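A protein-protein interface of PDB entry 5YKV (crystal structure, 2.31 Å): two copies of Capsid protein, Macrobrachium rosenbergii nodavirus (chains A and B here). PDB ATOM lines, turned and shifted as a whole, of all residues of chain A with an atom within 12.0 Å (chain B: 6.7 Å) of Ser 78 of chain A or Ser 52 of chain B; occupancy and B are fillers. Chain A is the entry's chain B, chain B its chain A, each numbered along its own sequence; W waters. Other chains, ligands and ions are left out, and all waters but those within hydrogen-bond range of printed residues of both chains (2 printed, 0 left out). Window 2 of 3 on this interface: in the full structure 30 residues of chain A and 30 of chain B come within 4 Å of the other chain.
Arg 50 of chain A touches Ser 78 of chain B, and with the chains exchanged Ser 78 of chain A touches Arg 50 of chain B.
Arg 50 of chain A touches Ile 80 of chain B, and with the chains exchanged Ile 80 of chain A touches Arg 50 of chain B.
Val 51 of chain A touches Ser 78 of chain B, and with the chains exchanged Ser 78 of chain A touches Val 51 of chain B.
Asp 76 of chain A touches Ile 80 of chain B, and with the chains exchanged Ile 80 of chain A touches Asp 76 of chain B.
12 positions are printed for both chains.
Of the 15 pairs that touch across the chains among the printed residues, 13 have their exchanged pair printed and touching as well.
Met 48 of chain A touches Ile 80 of chain B (SD to CG2, 3.5 Å).
Arg 50 of chain A touches Ser 78 of chain B.
O of Ser 78 of chain B touches CA of Val 51 of chain A (3.3 Å).
Ser 52 of chain A touches Ile 80 of chain B (CB to CD1, 3.7 Å).
Asp 76 of chain A touches Ile 80 of chain B (O to CD1, 3.8 Å).
Ser 78 of chain A touches Arg 50 of chain B (O to O, 3.8 Å).
Val 51 of chain B touches Ser 78 of chain A.
Arg 50 of chain B touches Ala 79 of chain A.
Ile 80 of chain A touches Asp 76 of chain B (CD1 to O, 3.5 Å).
Ile 80 of chain A touches Ile 80 of chain B (CD1 to CD1, 3.6 Å).
Of the printed residues of chain B, Met 48 of chain A touches Ile 80.
Printed residues of chain B within 4 Å of Ser 52 of chain A: Ser 78 (2.8 Å) and Ile 80 (3.7 Å).
Glu 54 of chain A touches none of the printed residues of chain B.
Ser 78 of chain A touches just these residues of chain B: Arg 50, Val 51 and Ser 52.
Cys 82 of chain A touches none of the printed residues of chain B.
Arg 50 of chain B touches three residues of chain A.
Of chain A, only Ser 78 comes within 4 Å of Val 51 of chain B.
Of chain A, only Ser 78 (2.8 Å) and Ile 80 (3.9 Å) come within 4 Å of Ser 52 of chain B.
No residue of chain A comes within 4 Å of Ser 53 of chain B.
No residue of chain A comes within 4 Å of Thr 77 of chain B.
The nearest residue of chain A that does not touch Ser 52 of chain B is Ala 79 of chain A (4.9 Å).
Water W1 bridges the backbone carbonyl oxygen (O) of Ile 80 of chain B (2.7 Å) and the backbone NH (N) of Arg 50 of chain A (3.2 Å).
Water W2 lies within hydrogen-bond range of O of Ser 52 of chain A (2.7 Å), OE2 of Glu 54 of chain A (2.8 Å) and OG of Ser 78 of chain B (3.2 Å).
Of the 12 printed residues of chain B, 6 touch a printed residue of chain A.
Printed residues of chain B that touch a printed residue of chain A: Arg 50, Val 51, Ser 52, Asp 76, Ser 78 and Ile 80.
Hydrophobic or aromatic side chains of chain B within 4 Å of the printed part of chain A: Ile 80.
Among the printed residues, 15 pairs touch across the chains.
Among the printed residues, no Asp or Glu carboxylate lies within 4 Å of a Lys or Arg side-chain nitrogen of the other chain.
The backbone carbonyl oxygen of Ser 78 of chain B sits at hydrogen-bond distance from the backbone NH of Ser 52 of chain A (2.8 Å).
N of Ser 52 of chain B sits at hydrogen-bond distance from O of Ser 78 of chain A.
The backbone carbonyl oxygen (O) of Arg 50 of chain B lies within hydrogen-bond range of the backbone NH (N) of Ile 80 of chain A (3.0 Å).
The backbone carbonyl oxygen (O) of Ile 80 of chain B lies within hydrogen-bond range of the backbone NH (N) of Arg 50 of chain A (3.1 Å).
The side-chain carboxylate (OD1) of Asp 76 of chain B sits at hydrogen-bond distance from the backbone NH (N) of Gln 57 of chain B (3.1 Å).
OE1 of Gln 57 of chain B is in hydrogen-bond range of NH2 of Arg 50 of chain B (2.8 Å).
The side-chain carboxylate (OD2) of Asp 76 of chain A lies within salt-bridge range of the guanidinium group (NH1) of Arg 50 of chain A.
The side-chain hydroxyl of Ser 52 of chain A is in hydrogen-bond range of the backbone carbonyl oxygen of Asp 76 of chain A (2.5 Å).
OE1 of Gln 57 of chain A sits at hydrogen-bond distance from NH2 of Arg 50 of chain A (2.8 Å).
OD1 of Asp 76 of chain A is in hydrogen-bond range of OG1 of Thr 77 of chain A (2.9 Å).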
ATOM      1  N   MET A  48      13.060 -12.357  -5.722  1.00  0.00           N
ATOM      2  CA  MET A  48      13.345 -13.642  -6.305  1.00  0.00           C
ATOM      3  C   MET A  48      12.028 -14.396  -6.506  1.00  0.00           C
ATOM      4  O   MET A  48      11.206 -14.525  -5.600  1.00  0.00           O
ATOM      5  CB  MET A  48      14.306 -14.439  -5.430  1.00  0.00           C
ATOM      6  CG  MET A  48      15.047 -15.482  -6.196  1.00  0.00           C
ATOM      7  SD  MET A  48      16.460 -16.216  -5.309  1.00  0.00           S
ATOM      8  CE  MET A  48      17.620 -14.855  -5.269  1.00  0.00           C
ATOM      9  N   ARG A  50      12.348 -17.656  -8.790  1.00  0.00           N
ATOM     10  CA  ARG A  50      13.428 -18.210  -9.633  1.00  0.00           C
ATOM     11  C   ARG A  50      13.885 -19.569  -9.093  1.00  0.00           C
ATOM     12  O   ARG A  50      14.277 -19.686  -7.923  1.00  0.00           O
ATOM     13  CB  ARG A  50      14.576 -17.202  -9.649  1.00  0.00           C
ATOM     14  CG  ARG A  50      15.783 -17.548 -10.504  1.00  0.00           C
ATOM     15  CD  ARG A  50      16.880 -16.573 -10.147  1.00  0.00           C
ATOM     16  NE  ARG A  50      18.092 -16.753 -10.938  1.00  0.00           N
ATOM     17  CZ  ARG A  50      19.067 -17.604 -10.621  1.00  0.00           C
ATOM     18  NH1 ARG A  50      18.899 -18.437  -9.601  1.00  0.00           N
ATOM     19  NH2 ARG A  50      20.172 -17.639 -11.350  1.00  0.00           N
ATOM     20  N   VAL A  51      13.850 -20.576  -9.970  1.00  0.00           N
ATOM     21  CA  VAL A  51      14.368 -21.879  -9.673  1.00  0.00           C
ATOM     22  C   VAL A  51      15.875 -21.742  -9.428  1.00  0.00           C
ATOM     23  O   VAL A  51      16.561 -21.032 -10.151  1.00  0.00           O
ATOM     24  CB  VAL A  51      14.017 -22.887 -10.784  1.00  0.00           C
ATOM     25  CG1 VAL A  51      14.709 -24.238 -10.594  1.00  0.00           C
ATOM     26  CG2 VAL A  51      12.502 -23.064 -10.883  1.00  0.00           C
ATOM     27  N   SER A  52      16.356 -22.323  -8.323  1.00  0.00           N
ATOM     28  CA  SER A  52      17.797 -22.331  -8.012  1.00  0.00           C
ATOM     29  C   SER A  52      18.537 -23.186  -9.053  1.00  0.00           C
ATOM     30  O   SER A  52      18.054 -24.253  -9.441  1.00  0.00           O
ATOM     31  CB  SER A  52      18.043 -22.852  -6.621  1.00  0.00           C
ATOM     32  OG  SER A  52      19.425 -23.022  -6.365  1.00  0.00           O
ATOM     33  N   SER A  53      19.701 -22.698  -9.488  1.00  0.00           N
ATOM     34  CA  SER A  53      20.573 -23.383 -10.428  1.00  0.00           C
ATOM     35  C   SER A  53      21.296 -24.526  -9.714  1.00  0.00           C
ATOM     36  O   SER A  53      21.765 -25.400 -10.339  1.00  0.00           O
ATOM     37  CB  SER A  53      21.594 -22.434 -11.029  1.00  0.00           C
ATOM     38  OG  SER A  53      22.526 -22.002 -10.035  1.00  0.00           O
ATOM     39  N   GLU A  54      21.477 -24.397  -8.404  1.00  0.00           N
ATOM     40  CA  GLU A  54      22.197 -25.346  -7.566  1.00  0.00           C
ATOM     41  C   GLU A  54      23.710 -25.298  -7.891  1.00  0.00           C
ATOM     42  O   GLU A  54      24.435 -26.086  -7.352  1.00  0.00           O
ATOM     43  CB  GLU A  54      21.559 -26.761  -7.642  1.00  0.00           C
ATOM     44  CG  GLU A  54      20.077 -26.873  -7.196  1.00  0.00           C
ATOM     45  CD  GLU A  54      19.585 -26.376  -5.804  1.00  0.00           C
ATOM     46  OE1 GLU A  54      20.433 -25.960  -4.953  1.00  0.00           O
ATOM     47  OE2 GLU A  54      18.306 -26.384  -5.534  1.00  0.00           O
ATOM     48  N   VAL A  55      24.185 -24.316  -8.687  1.00  0.00           N
ATOM     49  CA  VAL A  55      25.622 -24.175  -9.079  1.00  0.00           C
ATOM     50  C   VAL A  55      26.165 -22.769  -8.719  1.00  0.00           C
ATOM     51  O   VAL A  55      26.968 -22.194  -9.436  1.00  0.00           O
ATOM     52  CB  VAL A  55      25.874 -24.559 -10.563  1.00  0.00           C
ATOM     53  CG1 VAL A  55      25.566 -26.029 -10.829  1.00  0.00           C
ATOM     54  CG2 VAL A  55      25.107 -23.695 -11.555  1.00  0.00           C
ATOM     55  N   LEU A  56      25.779 -22.252  -7.550  1.00  0.00           N
ATOM     56  CA  LEU A  56      26.485 -21.181  -6.842  1.00  0.00           C
ATOM     57  C   LEU A  56      26.635 -19.948  -7.746  1.00  0.00           C
ATOM     58  O   LEU A  56      27.773 -19.506  -8.036  1.00  0.00           O
ATOM     59  CB  LEU A  56      27.848 -21.699  -6.342  1.00  0.00           C
ATOM     60  CG  LEU A  56      27.793 -22.691  -5.171  1.00  0.00           C
ATOM     61  CD1 LEU A  56      27.415 -24.093  -5.634  1.00  0.00           C
ATOM     62  CD2 LEU A  56      29.114 -22.730  -4.427  1.00  0.00           C
ATOM     63  N   GLN A  57      25.488 -19.410  -8.189  1.00  0.00           N
ATOM     64  CA  GLN A  57      25.470 -18.234  -9.063  1.00  0.00           C
ATOM     65  C   GLN A  57      25.410 -16.961  -8.216  1.00  0.00           C
ATOM     66  O   GLN A  57      24.371 -16.582  -7.693  1.00  0.00           O
ATOM     67  CB  GLN A  57      24.333 -18.357 -10.069  1.00  0.00           C
ATOM     68  CG  GLN A  57      24.581 -19.486 -11.052  1.00  0.00           C
ATOM     69  CD  GLN A  57      23.489 -19.683 -12.079  1.00  0.00           C
ATOM     70  OE1 GLN A  57      22.313 -19.378 -11.845  1.00  0.00           O
ATOM     71  NE2 GLN A  57      23.860 -20.330 -13.173  1.00  0.00           N
ATOM     72  N   LYS A  58      26.568 -16.343  -8.036  1.00  0.00           N
ATOM     73  CA  LYS A  58      26.738 -15.158  -7.202  1.00  0.00           C
ATOM     74  C   LYS A  58      26.780 -13.922  -8.115  1.00  0.00           C
ATOM     75  O   LYS A  58      27.469 -13.892  -9.127  1.00  0.00           O
ATOM     76  CB  LYS A  58      28.031 -15.250  -6.389  1.00  0.00           C
ATOM     77  CG  LYS A  58      28.399 -13.989  -5.622  1.00  0.00           C
ATOM     78  CD  LYS A  58      29.668 -14.114  -4.806  1.00  0.00           C
ATOM     79  CE  LYS A  58      29.909 -12.856  -3.997  1.00  0.00           C
ATOM     80  NZ  LYS A  58      31.228 -12.864  -3.325  1.00  0.00           N
ATOM     81  N   TYR A  74      22.914 -11.216  -4.792  1.00  0.00           N
ATOM     82  CA  TYR A  74      22.185 -12.431  -5.077  1.00  0.00           C
ATOM     83  C   TYR A  74      23.110 -13.640  -4.897  1.00  0.00           C
ATOM     84  O   TYR A  74      24.301 -13.579  -5.211  1.00  0.00           O
ATOM     85  CB  TYR A  74      21.662 -12.436  -6.509  1.00  0.00           C
ATOM     86  CG  TYR A  74      20.720 -11.310  -6.879  1.00  0.00           C
ATOM     87  CD1 TYR A  74      19.346 -11.431  -6.729  1.00  0.00           C
ATOM     88  CD2 TYR A  74      21.203 -10.128  -7.418  1.00  0.00           C
ATOM     89  CE1 TYR A  74      18.491 -10.380  -7.053  1.00  0.00           C
ATOM     90  CE2 TYR A  74      20.355  -9.096  -7.784  1.00  0.00           C
ATOM     91  CZ  TYR A  74      18.996  -9.218  -7.602  1.00  0.00           C
ATOM     92  OH  TYR A  74      18.191  -8.174  -7.946  1.00  0.00           O
ATOM     93  N   PHE A  75      22.538 -14.725  -4.366  1.00  0.00           N
ATOM     94  CA  PHE A  75      23.149 -16.044  -4.310  1.00  0.00           C
ATOM     95  C   PHE A  75      22.031 -17.081  -4.235  1.00  0.00           C
ATOM     96  O   PHE A  75      21.114 -16.896  -3.445  1.00  0.00           O
ATOM     97  CB  PHE A  75      24.072 -16.150  -3.099  1.00  0.00           C
ATOM     98  CG  PHE A  75      25.078 -17.244  -3.273  1.00  0.00           C
ATOM     99  CD1 PHE A  75      26.269 -16.998  -3.930  1.00  0.00           C
ATOM    100  CD2 PHE A  75      24.781 -18.543  -2.907  1.00  0.00           C
ATOM    101  CE1 PHE A  75      27.175 -18.027  -4.163  1.00  0.00           C
ATOM    102  CE2 PHE A  75      25.698 -19.566  -3.118  1.00  0.00           C
ATOM    103  CZ  PHE A  75      26.894 -19.311  -3.740  1.00  0.00           C
ATOM    104  N   ASP A  76      22.109 -18.170  -5.015  1.00  0.00           N
ATOM    105  CA  ASP A  76      20.964 -19.064  -5.155  1.00  0.00           C
ATOM    106  C   ASP A  76      21.135 -20.486  -4.592  1.00  0.00           C
ATOM    107  O   ASP A  76      20.174 -21.294  -4.736  1.00  0.00           O
ATOM    108  CB  ASP A  76      20.558 -19.164  -6.612  1.00  0.00           C
ATOM    109  CG  ASP A  76      21.507 -19.891  -7.530  1.00  0.00           C
ATOM    110  OD1 ASP A  76      22.686 -20.142  -7.116  1.00  0.00           O
ATOM    111  OD2 ASP A  76      21.065 -20.165  -8.682  1.00  0.00           O
ATOM    112  N   THR A  77      22.289 -20.826  -3.990  1.00  0.00           N
ATOM    113  CA  THR A  77      22.534 -22.215  -3.579  1.00  0.00           C
ATOM    114  C   THR A  77      22.822 -22.343  -2.085  1.00  0.00           C
ATOM    115  O   THR A  77      23.801 -21.789  -1.594  1.00  0.00           O
ATOM    116  CB  THR A  77      23.691 -22.852  -4.355  1.00  0.00           C
ATOM    117  OG1 THR A  77      23.440 -22.601  -5.742  1.00  0.00           O
ATOM    118  CG2 THR A  77      23.819 -24.342  -4.083  1.00  0.00           C
ATOM    119  N   SER A  78      21.973 -23.145  -1.416  1.00  0.00           N
ATOM    120  CA  SER A  78      22.005 -23.444   0.011  1.00  0.00           C
ATOM    121  C   SER A  78      21.817 -22.155   0.822  1.00  0.00           C
ATOM    122  O   SER A  78      20.725 -21.904   1.349  1.00  0.00           O
ATOM    123  CB  SER A  78      23.259 -24.217   0.384  1.00  0.00           C
ATOM    124  OG  SER A  78      23.264 -25.462  -0.298  1.00  0.00           O
ATOM    125  N   ALA A  79      22.872 -21.346   0.935  1.00  0.00           N
ATOM    126  CA  ALA A  79      22.793 -20.062   1.635  1.00  0.00           C
ATOM    127  C   ALA A  79      22.236 -18.990   0.687  1.00  0.00           C
ATOM    128  O   ALA A  79      22.980 -18.235   0.094  1.00  0.00           O
ATOM    129  CB  ALA A  79      24.145 -19.660   2.177  1.00  0.00           C
ATOM    130  N   ILE A  80      20.913 -18.900   0.615  1.00  0.00           N
ATOM    131  CA  ILE A  80      20.253 -18.043  -0.323  1.00  0.00           C
ATOM    132  C   ILE A  80      20.423 -16.592   0.102  1.00  0.00           C
ATOM    133  O   ILE A  80      20.202 -16.251   1.243  1.00  0.00           O
ATOM    134  CB  ILE A  80      18.767 -18.399  -0.451  1.00  0.00           C
ATOM    135  CG1 ILE A  80      18.625 -19.868  -0.845  1.00  0.00           C
ATOM    136  CG2 ILE A  80      18.077 -17.471  -1.442  1.00  0.00           C
ATOM    137  CD1 ILE A  80      17.229 -20.360  -0.705  1.00  0.00           C
ATOM    138  N   LYS A  81      20.742 -15.743  -0.878  1.00  0.00           N
ATOM    139  CA  LYS A  81      20.894 -14.328  -0.661  1.00  0.00           C
ATOM    140  C   LYS A  81      20.116 -13.580  -1.741  1.00  0.00           C
ATOM    141  O   LYS A  81      20.239 -13.856  -2.933  1.00  0.00           O
ATOM    142  CB  LYS A  81      22.373 -13.949  -0.679  1.00  0.00           C
ATOM    143  CG  LYS A  81      22.701 -12.640   0.008  1.00  0.00           C
ATOM    144  CD  LYS A  81      24.201 -12.436   0.195  1.00  0.00           C
ATOM    145  CE  LYS A  81      24.697 -12.698   1.595  1.00  0.00           C
ATOM    146  NZ  LYS A  81      26.027 -12.072   1.802  1.00  0.00           N
ATOM    147  N   CYS A  82      19.314 -12.640  -1.260  1.00  0.00           N
ATOM    148  CA  CYS A  82      18.498 -11.736  -2.017  1.00  0.00           C
ATOM    149  C   CYS A  82      18.378 -10.472  -1.167  1.00  0.00           C
ATOM    150  O   CYS A  82      17.396 -10.305  -0.491  1.00  0.00           O
ATOM    151  CB  CYS A  82      17.127 -12.344  -2.275  1.00  0.00           C
ATOM    152  SG  CYS A  82      16.007 -11.273  -3.216  1.00  0.00           S
ATOM    153  N   GLN A 105      29.458 -20.814 -10.629  1.00  0.00           N
ATOM    154  CA  GLN A 105      30.226 -22.090 -10.763  1.00  0.00           C
ATOM    155  C   GLN A 105      29.889 -22.756 -12.109  1.00  0.00           C
ATOM    156  O   GLN A 105      30.734 -23.346 -12.720  1.00  0.00           O
ATOM    157  CB  GLN A 105      29.880 -23.009  -9.595  1.00  0.00           C
ATOM    158  CG  GLN A 105      30.758 -24.234  -9.430  1.00  0.00           C
ATOM    159  CD  GLN A 105      30.123 -25.250  -8.497  1.00  0.00           C
ATOM    160  OE1 GLN A 105      29.136 -25.923  -8.858  1.00  0.00           O
ATOM    161  NE2 GLN A 105      30.655 -25.330  -7.277  1.00  0.00           N
ATOM    162  N   TYR A 113      18.635 -12.860 -12.545  1.00  0.00           N
ATOM    163  CA  TYR A 113      18.243 -12.331 -11.241  1.00  0.00           C
ATOM    164  C   TYR A 113      17.319 -11.125 -11.483  1.00  0.00           C
ATOM    165  O   TYR A 113      17.423 -10.503 -12.532  1.00  0.00           O
ATOM    166  CB  TYR A 113      19.484 -12.018 -10.403  1.00  0.00           C
ATOM    167  CG  TYR A 113      20.149 -13.249  -9.837  1.00  0.00           C
ATOM    168  CD1 TYR A 113      19.461 -14.067  -8.960  1.00  0.00           C
ATOM    169  CD2 TYR A 113      21.449 -13.613 -10.175  1.00  0.00           C
ATOM    170  CE1 TYR A 113      20.056 -15.182  -8.387  1.00  0.00           C
ATOM    171  CE2 TYR A 113      22.046 -14.738  -9.628  1.00  0.00           C
ATOM    172  CZ  TYR A 113      21.340 -15.533  -8.743  1.00  0.00           C
ATOM    173  OH  TYR A 113      21.872 -16.641  -8.182  1.00  0.00           O
ATOM    174  N   ARG B  50      19.761 -16.331   4.292  1.00  0.00           N
ATOM    175  CA  ARG B  50      19.188 -17.428   5.043  1.00  0.00           C
ATOM    176  C   ARG B  50      19.518 -18.746   4.348  1.00  0.00           C
ATOM    177  O   ARG B  50      19.235 -18.924   3.117  1.00  0.00           O
ATOM    178  CB  ARG B  50      17.672 -17.219   5.100  1.00  0.00           C
ATOM    179  CG  ARG B  50      16.889 -18.296   5.827  1.00  0.00           C
ATOM    180  CD  ARG B  50      15.416 -17.966   5.701  1.00  0.00           C
ATOM    181  NE  ARG B  50      14.587 -18.885   6.443  1.00  0.00           N
ATOM    182  CZ  ARG B  50      14.086 -20.031   5.972  1.00  0.00           C
ATOM    183  NH1 ARG B  50      14.557 -20.583   4.859  1.00  0.00           N
ATOM    184  NH2 ARG B  50      13.074 -20.589   6.615  1.00  0.00           N
ATOM    185  N   VAL B  51      20.071 -19.674   5.143  1.00  0.00           N
ATOM    186  CA  VAL B  51      20.306 -21.043   4.688  1.00  0.00           C
ATOM    187  C   VAL B  51      18.935 -21.691   4.497  1.00  0.00           C
ATOM    188  O   VAL B  51      18.066 -21.578   5.322  1.00  0.00           O
ATOM    189  CB  VAL B  51      21.192 -21.840   5.670  1.00  0.00           C
ATOM    190  CG1 VAL B  51      21.323 -23.304   5.260  1.00  0.00           C
ATOM    191  CG2 VAL B  51      22.573 -21.211   5.842  1.00  0.00           C
ATOM    192  N   SER B  52      18.755 -22.345   3.356  1.00  0.00           N
ATOM    193  CA  SER B  52      17.537 -23.051   3.014  1.00  0.00           C
ATOM    194  C   SER B  52      17.371 -24.259   3.933  1.00  0.00           C
ATOM    195  O   SER B  52      18.349 -24.953   4.179  1.00  0.00           O
ATOM    196  CB  SER B  52      17.573 -23.490   1.560  1.00  0.00           C
ATOM    197  OG  SER B  52      16.493 -24.363   1.256  1.00  0.00           O
ATOM    198  N   SER B  53      16.134 -24.530   4.366  1.00  0.00           N
ATOM    199  CA  SER B  53      15.796 -25.709   5.178  1.00  0.00           C
ATOM    200  C   SER B  53      15.832 -26.993   4.327  1.00  0.00           C
ATOM    201  O   SER B  53      15.923 -28.067   4.849  1.00  0.00           O
ATOM    202  CB  SER B  53      14.441 -25.508   5.815  1.00  0.00           C
ATOM    203  OG  SER B  53      13.397 -25.483   4.831  1.00  0.00           O
ATOM    204  N   GLU B  54      15.713 -26.847   3.000  1.00  0.00           N
ATOM    205  CA  GLU B  54      15.512 -27.911   1.994  1.00  0.00           C
ATOM    206  C   GLU B  54      14.223 -28.711   2.281  1.00  0.00           C
ATOM    207  O   GLU B  54      14.003 -29.717   1.627  1.00  0.00           O
ATOM    208  CB  GLU B  54      16.737 -28.828   1.834  1.00  0.00           C
ATOM    209  CG  GLU B  54      18.029 -28.171   1.333  1.00  0.00           C
ATOM    210  CD  GLU B  54      18.032 -27.132   0.184  1.00  0.00           C
ATOM    211  OE1 GLU B  54      17.126 -27.132  -0.725  1.00  0.00           O
ATOM    212  OE2 GLU B  54      18.977 -26.289   0.171  1.00  0.00           O
ATOM    213  N   VAL B  55      13.331 -28.218   3.160  1.00  0.00           N
ATOM    214  CA  VAL B  55      12.060 -28.907   3.461  1.00  0.00           C
ATOM    215  C   VAL B  55      10.840 -27.987   3.215  1.00  0.00           C
ATOM    216  O   VAL B  55       9.873 -28.003   3.988  1.00  0.00           O
ATOM    217  CB  VAL B  55      12.062 -29.493   4.884  1.00  0.00           C
ATOM    218  CG1 VAL B  55      13.118 -30.581   5.039  1.00  0.00           C
ATOM    219  CG2 VAL B  55      12.226 -28.432   5.956  1.00  0.00           C
ATOM    220  N   LEU B  56      10.861 -27.197   2.128  1.00  0.00           N
ATOM    221  CA  LEU B  56       9.643 -26.597   1.552  1.00  0.00           C
ATOM    222  C   LEU B  56       8.890 -25.722   2.578  1.00  0.00           C
ATOM    223  O   LEU B  56       7.660 -25.918   2.846  1.00  0.00           O
ATOM    224  CB  LEU B  56       8.744 -27.705   0.980  1.00  0.00           C
ATOM    225  CG  LEU B  56       9.286 -28.393  -0.279  1.00  0.00           C
ATOM    226  CD1 LEU B  56      10.409 -29.359   0.086  1.00  0.00           C
ATOM    227  CD2 LEU B  56       8.196 -29.128  -1.055  1.00  0.00           C
ATOM    228  N   GLN B  57       9.570 -24.673   3.051  1.00  0.00           N
ATOM    229  CA  GLN B  57       8.975 -23.751   4.039  1.00  0.00           C
ATOM    230  C   GLN B  57       8.332 -22.556   3.316  1.00  0.00           C
ATOM    231  O   GLN B  57       8.986 -21.581   2.952  1.00  0.00           O
ATOM    232  CB  GLN B  57      10.022 -23.365   5.089  1.00  0.00           C
ATOM    233  CG  GLN B  57      10.490 -24.582   5.875  1.00  0.00           C
ATOM    234  CD  GLN B  57      11.545 -24.311   6.907  1.00  0.00           C
ATOM    235  OE1 GLN B  57      12.233 -23.296   6.866  1.00  0.00           O
ATOM    236  NE2 GLN B  57      11.649 -25.221   7.858  1.00  0.00           N
ATOM    237  N   ASP B  76      11.741 -21.504   0.194  1.00  0.00           N
ATOM    238  CA  ASP B  76      13.185 -21.638   0.338  1.00  0.00           C
ATOM    239  C   ASP B  76      13.761 -22.845  -0.408  1.00  0.00           C
ATOM    240  O   ASP B  76      14.958 -23.016  -0.390  1.00  0.00           O
ATOM    241  CB  ASP B  76      13.582 -21.712   1.811  1.00  0.00           C
ATOM    242  CG  ASP B  76      13.162 -22.959   2.570  1.00  0.00           C
ATOM    243  OD1 ASP B  76      12.330 -23.739   2.064  1.00  0.00           O
ATOM    244  OD2 ASP B  76      13.664 -23.119   3.685  1.00  0.00           O
ATOM    245  N   THR B  77      12.937 -23.677  -1.052  1.00  0.00           N
ATOM    246  CA  THR B  77      13.405 -24.989  -1.616  1.00  0.00           C
ATOM    247  C   THR B  77      13.179 -25.080  -3.138  1.00  0.00           C
ATOM    248  O   THR B  77      12.039 -25.159  -3.633  1.00  0.00           O
ATOM    249  CB  THR B  77      12.703 -26.168  -0.921  1.00  0.00           C
ATOM    250  OG1 THR B  77      12.944 -26.046   0.481  1.00  0.00           O
ATOM    251  CG2 THR B  77      13.186 -27.515  -1.420  1.00  0.00           C
ATOM    252  N   SER B  78      14.284 -25.080  -3.885  1.00  0.00           N
ATOM    253  CA  SER B  78      14.308 -25.235  -5.331  1.00  0.00           C
ATOM    254  C   SER B  78      13.644 -24.044  -6.057  1.00  0.00           C
ATOM    255  O   SER B  78      14.326 -23.238  -6.674  1.00  0.00           O
ATOM    256  CB  SER B  78      13.699 -26.556  -5.753  1.00  0.00           C
ATOM    257  OG  SER B  78      13.767 -26.656  -7.165  1.00  0.00           O
ATOM    258  N   ILE B  80      12.614 -20.893  -5.632  1.00  0.00           N
ATOM    259  CA  ILE B  80      12.776 -19.927  -4.555  1.00  0.00           C
ATOM    260  C   ILE B  80      11.860 -18.698  -4.734  1.00  0.00           C
ATOM    261  O   ILE B  80      11.760 -18.138  -5.822  1.00  0.00           O
ATOM    262  CB  ILE B  80      14.248 -19.538  -4.458  1.00  0.00           C
ATOM    263  CG1 ILE B  80      15.043 -20.797  -4.112  1.00  0.00           C
ATOM    264  CG2 ILE B  80      14.412 -18.412  -3.443  1.00  0.00           C
ATOM    265  CD1 ILE B  80      16.489 -20.597  -4.178  1.00  0.00           C
HETATM  266  O   HOH W   1      10.041 -19.400  -7.540  1.00  0.00           O
HETATM  267  O   HOH W   2      16.854 -26.207  -7.942  1.00  0.00           O
